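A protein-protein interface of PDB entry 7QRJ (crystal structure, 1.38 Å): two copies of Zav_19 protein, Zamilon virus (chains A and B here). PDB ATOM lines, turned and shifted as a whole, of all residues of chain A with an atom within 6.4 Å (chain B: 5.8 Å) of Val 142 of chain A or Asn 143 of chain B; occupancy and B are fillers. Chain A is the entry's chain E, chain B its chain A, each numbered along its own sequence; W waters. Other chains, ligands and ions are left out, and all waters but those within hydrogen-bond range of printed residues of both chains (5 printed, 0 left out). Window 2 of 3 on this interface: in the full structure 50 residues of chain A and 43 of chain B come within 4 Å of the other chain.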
ATOM      1  N   ARG A 140       6.625   4.745   2.588  1.00  0.00           N
ATOM      2  CA  ARG A 140       6.173   3.413   2.205  1.00  0.00           C
ATOM      3  C   ARG A 140       7.332   2.686   1.533  1.00  0.00           C
ATOM      4  O   ARG A 140       7.477   2.742   0.302  1.00  0.00           O
ATOM      5  CB  ARG A 140       4.976   3.529   1.254  1.00  0.00           C
ATOM      6  CG  ARG A 140       3.807   4.340   1.813  1.00  0.00           C
ATOM      7  CD  ARG A 140       2.749   4.624   0.753  1.00  0.00           C
ATOM      8  NE  ARG A 140       2.204   3.382   0.202  1.00  0.00           N
ATOM      9  CZ  ARG A 140       1.072   2.808   0.598  1.00  0.00           C
ATOM     10  NH1 ARG A 140       0.339   3.324   1.577  1.00  0.00           N
ATOM     11  NH2 ARG A 140       0.656   1.697  -0.010  1.00  0.00           N
ATOM     12  N   PRO A 141       8.198   2.005   2.291  1.00  0.00           N
ATOM     13  CA  PRO A 141       9.404   1.418   1.687  1.00  0.00           C
ATOM     14  C   PRO A 141       9.075   0.271   0.748  1.00  0.00           C
ATOM     15  O   PRO A 141       8.134  -0.491   0.979  1.00  0.00           O
ATOM     16  CB  PRO A 141      10.206   0.925   2.897  1.00  0.00           C
ATOM     17  CG  PRO A 141       9.182   0.703   3.962  1.00  0.00           C
ATOM     18  CD  PRO A 141       8.127   1.753   3.742  1.00  0.00           C
ATOM     19  N   VAL A 142       9.878   0.146  -0.315  1.00  0.00           N
ATOM     20  CA  VAL A 142       9.626  -0.884  -1.319  1.00  0.00           C
ATOM     21  C   VAL A 142      10.045  -2.266  -0.835  1.00  0.00           C
ATOM     22  O   VAL A 142       9.466  -3.268  -1.258  1.00  0.00           O
ATOM     23  CB  VAL A 142      10.254  -0.534  -2.680  1.00  0.00           C
ATOM     24  CG1 VAL A 142       9.555   0.669  -3.298  1.00  0.00           C
ATOM     25  CG2 VAL A 142      11.767  -0.332  -2.557  1.00  0.00           C
ATOM     26  N   ASN A 143      11.049  -2.363   0.037  1.00  0.00           N
ATOM     27  CA  ASN A 143      11.382  -3.664   0.610  1.00  0.00           C
ATOM     28  C   ASN A 143      10.268  -4.113   1.549  1.00  0.00           C
ATOM     29  O   ASN A 143       9.735  -3.302   2.310  1.00  0.00           O
ATOM     30  CB  ASN A 143      12.690  -3.602   1.399  1.00  0.00           C
ATOM     31  CG  ASN A 143      13.897  -3.318   0.526  1.00  0.00           C
ATOM     32  OD1 ASN A 143      13.904  -3.610  -0.668  1.00  0.00           O
ATOM     33  ND2 ASN A 143      14.937  -2.760   1.129  1.00  0.00           N
ATOM     34  N   PRO A 144       9.914  -5.395   1.542  1.00  0.00           N
ATOM     35  CA  PRO A 144       8.910  -5.874   2.500  1.00  0.00           C
ATOM     36  C   PRO A 144       9.441  -5.846   3.925  1.00  0.00           C
ATOM     37  O   PRO A 144      10.628  -6.065   4.183  1.00  0.00           O
ATOM     38  CB  PRO A 144       8.668  -7.323   2.062  1.00  0.00           C
ATOM     39  CG  PRO A 144       9.977  -7.723   1.395  1.00  0.00           C
ATOM     40  CD  PRO A 144      10.444  -6.476   0.690  1.00  0.00           C
ATOM     41  N   GLU B 131       1.521  -8.247   0.291  1.00  0.00           N
ATOM     42  CA  GLU B 131       2.628  -8.268  -0.662  1.00  0.00           C
ATOM     43  C   GLU B 131       2.422  -9.390  -1.668  1.00  0.00           C
ATOM     44  O   GLU B 131       2.226 -10.550  -1.285  1.00  0.00           O
ATOM     45  CB  GLU B 131       3.948  -8.510   0.071  1.00  0.00           C
ATOM     46  CG  GLU B 131       4.275  -7.504   1.159  1.00  0.00           C
ATOM     47  CD  GLU B 131       4.726  -6.173   0.600  1.00  0.00           C
ATOM     48  OE1 GLU B 131       4.002  -5.600  -0.252  1.00  0.00           O
ATOM     49  OE2 GLU B 131       5.795  -5.672   0.994  1.00  0.00           O
ATOM     50  N   ILE B 132       2.496  -9.050  -2.959  1.00  0.00           N
ATOM     51  CA  ILE B 132       2.292 -10.015  -4.033  1.00  0.00           C
ATOM     52  C   ILE B 132       3.307  -9.751  -5.139  1.00  0.00           C
ATOM     53  O   ILE B 132       3.824  -8.645  -5.285  1.00  0.00           O
ATOM     54  CB  ILE B 132       0.853  -9.973  -4.614  1.00  0.00           C
ATOM     55  CG1 ILE B 132       0.514  -8.567  -5.129  1.00  0.00           C
ATOM     56  CG2 ILE B 132      -0.165 -10.464  -3.579  1.00  0.00           C
ATOM     57  CD1 ILE B 132      -0.726  -8.525  -6.015  1.00  0.00           C
ATOM     58  N   VAL B 134       4.225  -8.992  -8.836  1.00  0.00           N
ATOM     59  CA  VAL B 134       3.643  -8.365 -10.022  1.00  0.00           C
ATOM     60  C   VAL B 134       4.692  -8.256 -11.131  1.00  0.00           C
ATOM     61  O   VAL B 134       5.899  -8.346 -10.895  1.00  0.00           O
ATOM     62  CB  VAL B 134       3.028  -6.976  -9.724  1.00  0.00           C
ATOM     63  CG1 VAL B 134       1.928  -7.099  -8.691  1.00  0.00           C
ATOM     64  CG2 VAL B 134       4.092  -5.980  -9.298  1.00  0.00           C
ATOM     65  N   PRO B 141       9.951  -7.533 -11.534  1.00  0.00           N
ATOM     66  CA  PRO B 141      10.683  -6.669 -10.601  1.00  0.00           C
ATOM     67  C   PRO B 141      10.914  -7.356  -9.266  1.00  0.00           C
ATOM     68  O   PRO B 141      10.080  -8.131  -8.788  1.00  0.00           O
ATOM     69  CB  PRO B 141       9.766  -5.449 -10.448  1.00  0.00           C
ATOM     70  CG  PRO B 141       8.404  -5.963 -10.783  1.00  0.00           C
ATOM     71  CD  PRO B 141       8.611  -7.000 -11.845  1.00  0.00           C
ATOM     72  N   VAL B 142      12.066  -7.055  -8.658  1.00  0.00           N
ATOM     73  CA  VAL B 142      12.407  -7.657  -7.373  1.00  0.00           C
ATOM     74  C   VAL B 142      11.571  -7.083  -6.230  1.00  0.00           C
ATOM     75  O   VAL B 142      11.319  -7.777  -5.242  1.00  0.00           O
ATOM     76  CB  VAL B 142      13.919  -7.586  -7.092  1.00  0.00           C
ATOM     77  CG1 VAL B 142      14.688  -8.489  -8.064  1.00  0.00           C
ATOM     78  CG2 VAL B 142      14.430  -6.146  -7.136  1.00  0.00           C
ATOM     79  N   ASN B 143      11.142  -5.825  -6.322  1.00  0.00           N
ATOM     80  CA  ASN B 143      10.268  -5.285  -5.287  1.00  0.00           C
ATOM     81  C   ASN B 143       8.880  -5.911  -5.392  1.00  0.00           C
ATOM     82  O   ASN B 143       8.359  -6.097  -6.499  1.00  0.00           O
ATOM     83  CB  ASN B 143      10.120  -3.771  -5.412  1.00  0.00           C
ATOM     84  CG  ASN B 143      11.411  -3.035  -5.192  1.00  0.00           C
ATOM     85  OD1 ASN B 143      12.304  -3.517  -4.494  1.00  0.00           O
ATOM     86  ND2 ASN B 143      11.503  -1.835  -5.747  1.00  0.00           N
ATOM     87  N   PRO B 144       8.250  -6.236  -4.266  1.00  0.00           N
ATOM     88  CA  PRO B 144       6.885  -6.765  -4.323  1.00  0.00           C
ATOM     89  C   PRO B 144       5.897  -5.705  -4.783  1.00  0.00           C
ATOM     90  O   PRO B 144       6.063  -4.507  -4.529  1.00  0.00           O
ATOM     91  CB  PRO B 144       6.602  -7.167  -2.871  1.00  0.00           C
ATOM     92  CG  PRO B 144       7.498  -6.248  -2.058  1.00  0.00           C
ATOM     93  CD  PRO B 144       8.751  -6.112  -2.884  1.00  0.00           C
ATOM     94  N   GLY B 145       4.856  -6.167  -5.475  1.00  0.00           N
ATOM     95  CA  GLY B 145       3.657  -5.372  -5.627  1.00  0.00           C
ATOM     96  C   GLY B 145       2.810  -5.404  -4.363  1.00  0.00           C
ATOM     97  O   GLY B 145       3.092  -6.125  -3.405  1.00  0.00           O
ATOM     98  N   LYS B 159       2.119  -1.388  -8.433  1.00  0.00           N
ATOM     99  CA  LYS B 159       3.364  -1.965  -8.930  1.00  0.00           C
ATOM    100  C   LYS B 159       4.381  -2.176  -7.813  1.00  0.00           C
ATOM    101  O   LYS B 159       5.181  -3.115  -7.881  1.00  0.00           O
ATOM    102  CB  LYS B 159       3.923  -1.081 -10.046  1.00  0.00           C
ATOM    103  CG  LYS B 159       5.048  -1.709 -10.863  1.00  0.00           C
ATOM    104  CD  LYS B 159       6.406  -1.240 -10.395  1.00  0.00           C
ATOM    105  CE  LYS B 159       7.513  -1.876 -11.233  1.00  0.00           C
ATOM    106  NZ  LYS B 159       7.506  -1.445 -12.663  1.00  0.00           N
ATOM    107  N   ASP B 160       4.371  -1.323  -6.788  1.00  0.00           N
ATOM    108  CA  ASP B 160       5.236  -1.503  -5.625  1.00  0.00           C
ATOM    109  C   ASP B 160       4.522  -0.944  -4.399  1.00  0.00           C
ATOM    110  O   ASP B 160       3.398  -0.445  -4.489  1.00  0.00           O
ATOM    111  CB  ASP B 160       6.638  -0.898  -5.829  1.00  0.00           C
ATOM    112  CG  ASP B 160       6.614   0.596  -6.085  1.00  0.00           C
ATOM    113  OD1 ASP B 160       5.759   1.295  -5.507  1.00  0.00           O
ATOM    114  OD2 ASP B 160       7.485   1.090  -6.842  1.00  0.00           O
ATOM    115  N   ASN B 161       5.195  -1.013  -3.243  1.00  0.00           N
ATOM    116  CA  ASN B 161       4.591  -0.554  -1.995  1.00  0.00           C
ATOM    117  C   ASN B 161       4.426   0.956  -1.930  1.00  0.00           C
ATOM    118  O   ASN B 161       3.704   1.445  -1.053  1.00  0.00           O
ATOM    119  CB  ASN B 161       5.440  -0.962  -0.791  1.00  0.00           C
ATOM    120  CG  ASN B 161       5.448  -2.450  -0.549  1.00  0.00           C
ATOM    121  OD1 ASN B 161       4.563  -3.178  -1.016  1.00  0.00           O
ATOM    122  ND2 ASN B 161       6.456  -2.918   0.175  1.00  0.00           N
ATOM    123  N   ASN B 162       5.094   1.701  -2.802  1.00  0.00           N
ATOM    124  CA  ASN B 162       5.101   3.165  -2.734  1.00  0.00           C
ATOM    125  C   ASN B 162       4.130   3.779  -3.732  1.00  0.00           C
ATOM    126  O   ASN B 162       4.465   4.723  -4.452  1.00  0.00           O
ATOM    127  CB  ASN B 162       6.513   3.696  -2.942  1.00  0.00           C
ATOM    128  CG  ASN B 162       6.641   5.151  -2.558  1.00  0.00           C
ATOM    129  OD1 ASN B 162       5.893   5.639  -1.712  1.00  0.00           O
ATOM    130  ND2 ASN B 162       7.559   5.860  -3.210  1.00  0.00           N
HETATM  131  O   HOH W   1       7.202  -2.583   3.376  1.00  0.00           O
HETATM  132  O   HOH W   2       6.906   6.822   0.538  1.00  0.00           O
HETATM  133  O   HOH W   3       7.531  -2.676  -3.187  1.00  0.00           O
HETATM  134  O   HOH W   4      12.542  -5.418  -2.400  1.00  0.00           O
HETATM  135  O   HOH W   5       1.453   0.879  -2.915  1.00  0.00           O
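Water W3 lies within hydrogen-bond range of the backbone carbonyl oxygen of Pro 144 of chain B (2.7 Å), the backbone carbonyl oxygen of Val 142 of chain A (2.8 Å) and the backbone NH of Asn 161 of chain B (2.9 Å).
Water W2 bridges OD1 of Asn 162 of chain B (2.7 Å) and N of Arg 140 of chain A (2.9 Å).
Water W5 lies within hydrogen-bond range of O of Asp 160 of chain B (2.8 Å), O of Asn 161 of chain B (3.0 Å) and NH2 of Arg 140 of chain A (3.1 Å).
Water W4 lies within hydrogen-bond range of OD1 of Asn 143 of chain B and OD1 of Asn 143 of chain A.
Water W1 lies within hydrogen-bond range of the backbone carbonyl oxygen (O) of Asn 143 of chain A, the side-chain amide nitrogen (ND2) of Asn 161 of chain B and the backbone carbonyl oxygen (O) of Pro 141 of chain A.
Among the printed residues, merely in contact across the chains: Val 142 of chain A with Pro 144 of chain B (3.4 Å), Pro 144 of chain A with Glu 131 of chain B (3.5 Å), Arg 140 of chain A with Asn 162 of chain B (3.5 Å), Val 142 of chain A with Asn 143 of chain B (3.5 Å), Asn 143 of chain A with Asn 161 of chain B (3.9 Å) and Pro 144 of chain A with Pro 144 of chain B (3.97 Å).
Val 142 of chain A touches three residues of chain B.
Printed residues of chain A within 4 Å of Glu 131 of chain B: Pro 144 (3.5 Å).
Printed residues of chain A within 4 Å of Asn 143 of chain B: Val 142.
Of the printed residues of chain A, Pro 144 of chain B touches Val 142 (3.4 Å) and Pro 144 (3.97 Å).
The nearest residue of chain A that does not touch Asn 143 of chain B is Asn 143 of chain A (4.1 Å).
The nearest printed residue of chain B that does not touch Pro 141 of chain A is Asn 162 of chain B (5.3 Å).
OD1 of Asn 161 of chain B lies close to OE1 of Glu 131 of chain B (2.6 Å).
The side-chain carboxylate (OD1) of Asp 160 of chain B sits at hydrogen-bond distance from the backbone NH (N) of Asn 162 of chain B, 2.8 Å away.
Printed residues of chain B that touch a printed residue of chain A: Glu 131, Asn 143, Pro 144, Asn 161 and Asn 162.
Hydrophobic or aromatic side chains of chain B within 4 Å of the printed part of chain A: Pro 144.
Hydrophobic or aromatic side chains of chain A that line the printed part of chain B: Val 142 and Pro 144.
Among the printed residues, 9 pairs touch across the chains.
ND2 of Asn 161 of chain B is in hydrogen-bond range of O of Val 142 of chain A (3.4 Å).
NE of Arg 140 of chain A is in hydrogen-bond range of O of Asn 161 of chain B (2.8 Å).
The side-chain amide nitrogen of Asn 161 of chain B lies within hydrogen-bond range of the backbone carbonyl oxygen of Pro 141 of chain A, 3.1 Å away.
Val 142 of chain A touches Asn 143 of chain B, but with the chains exchanged Asn 143 of chain A does not touch Val 142 of chain B (6.7 Å).
Val 142 of chain A touches Pro 144 of chain B, but with the chains exchanged Pro 144 of chain A does not touch Val 142 of chain B (6.1 Å).
Pro 144 of chain A touches its own counterpart, Pro 144 of chain B.
Of the 9 pairs that touch across the chains among the printed residues, 1 has its exchanged pair printed and touching as well.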
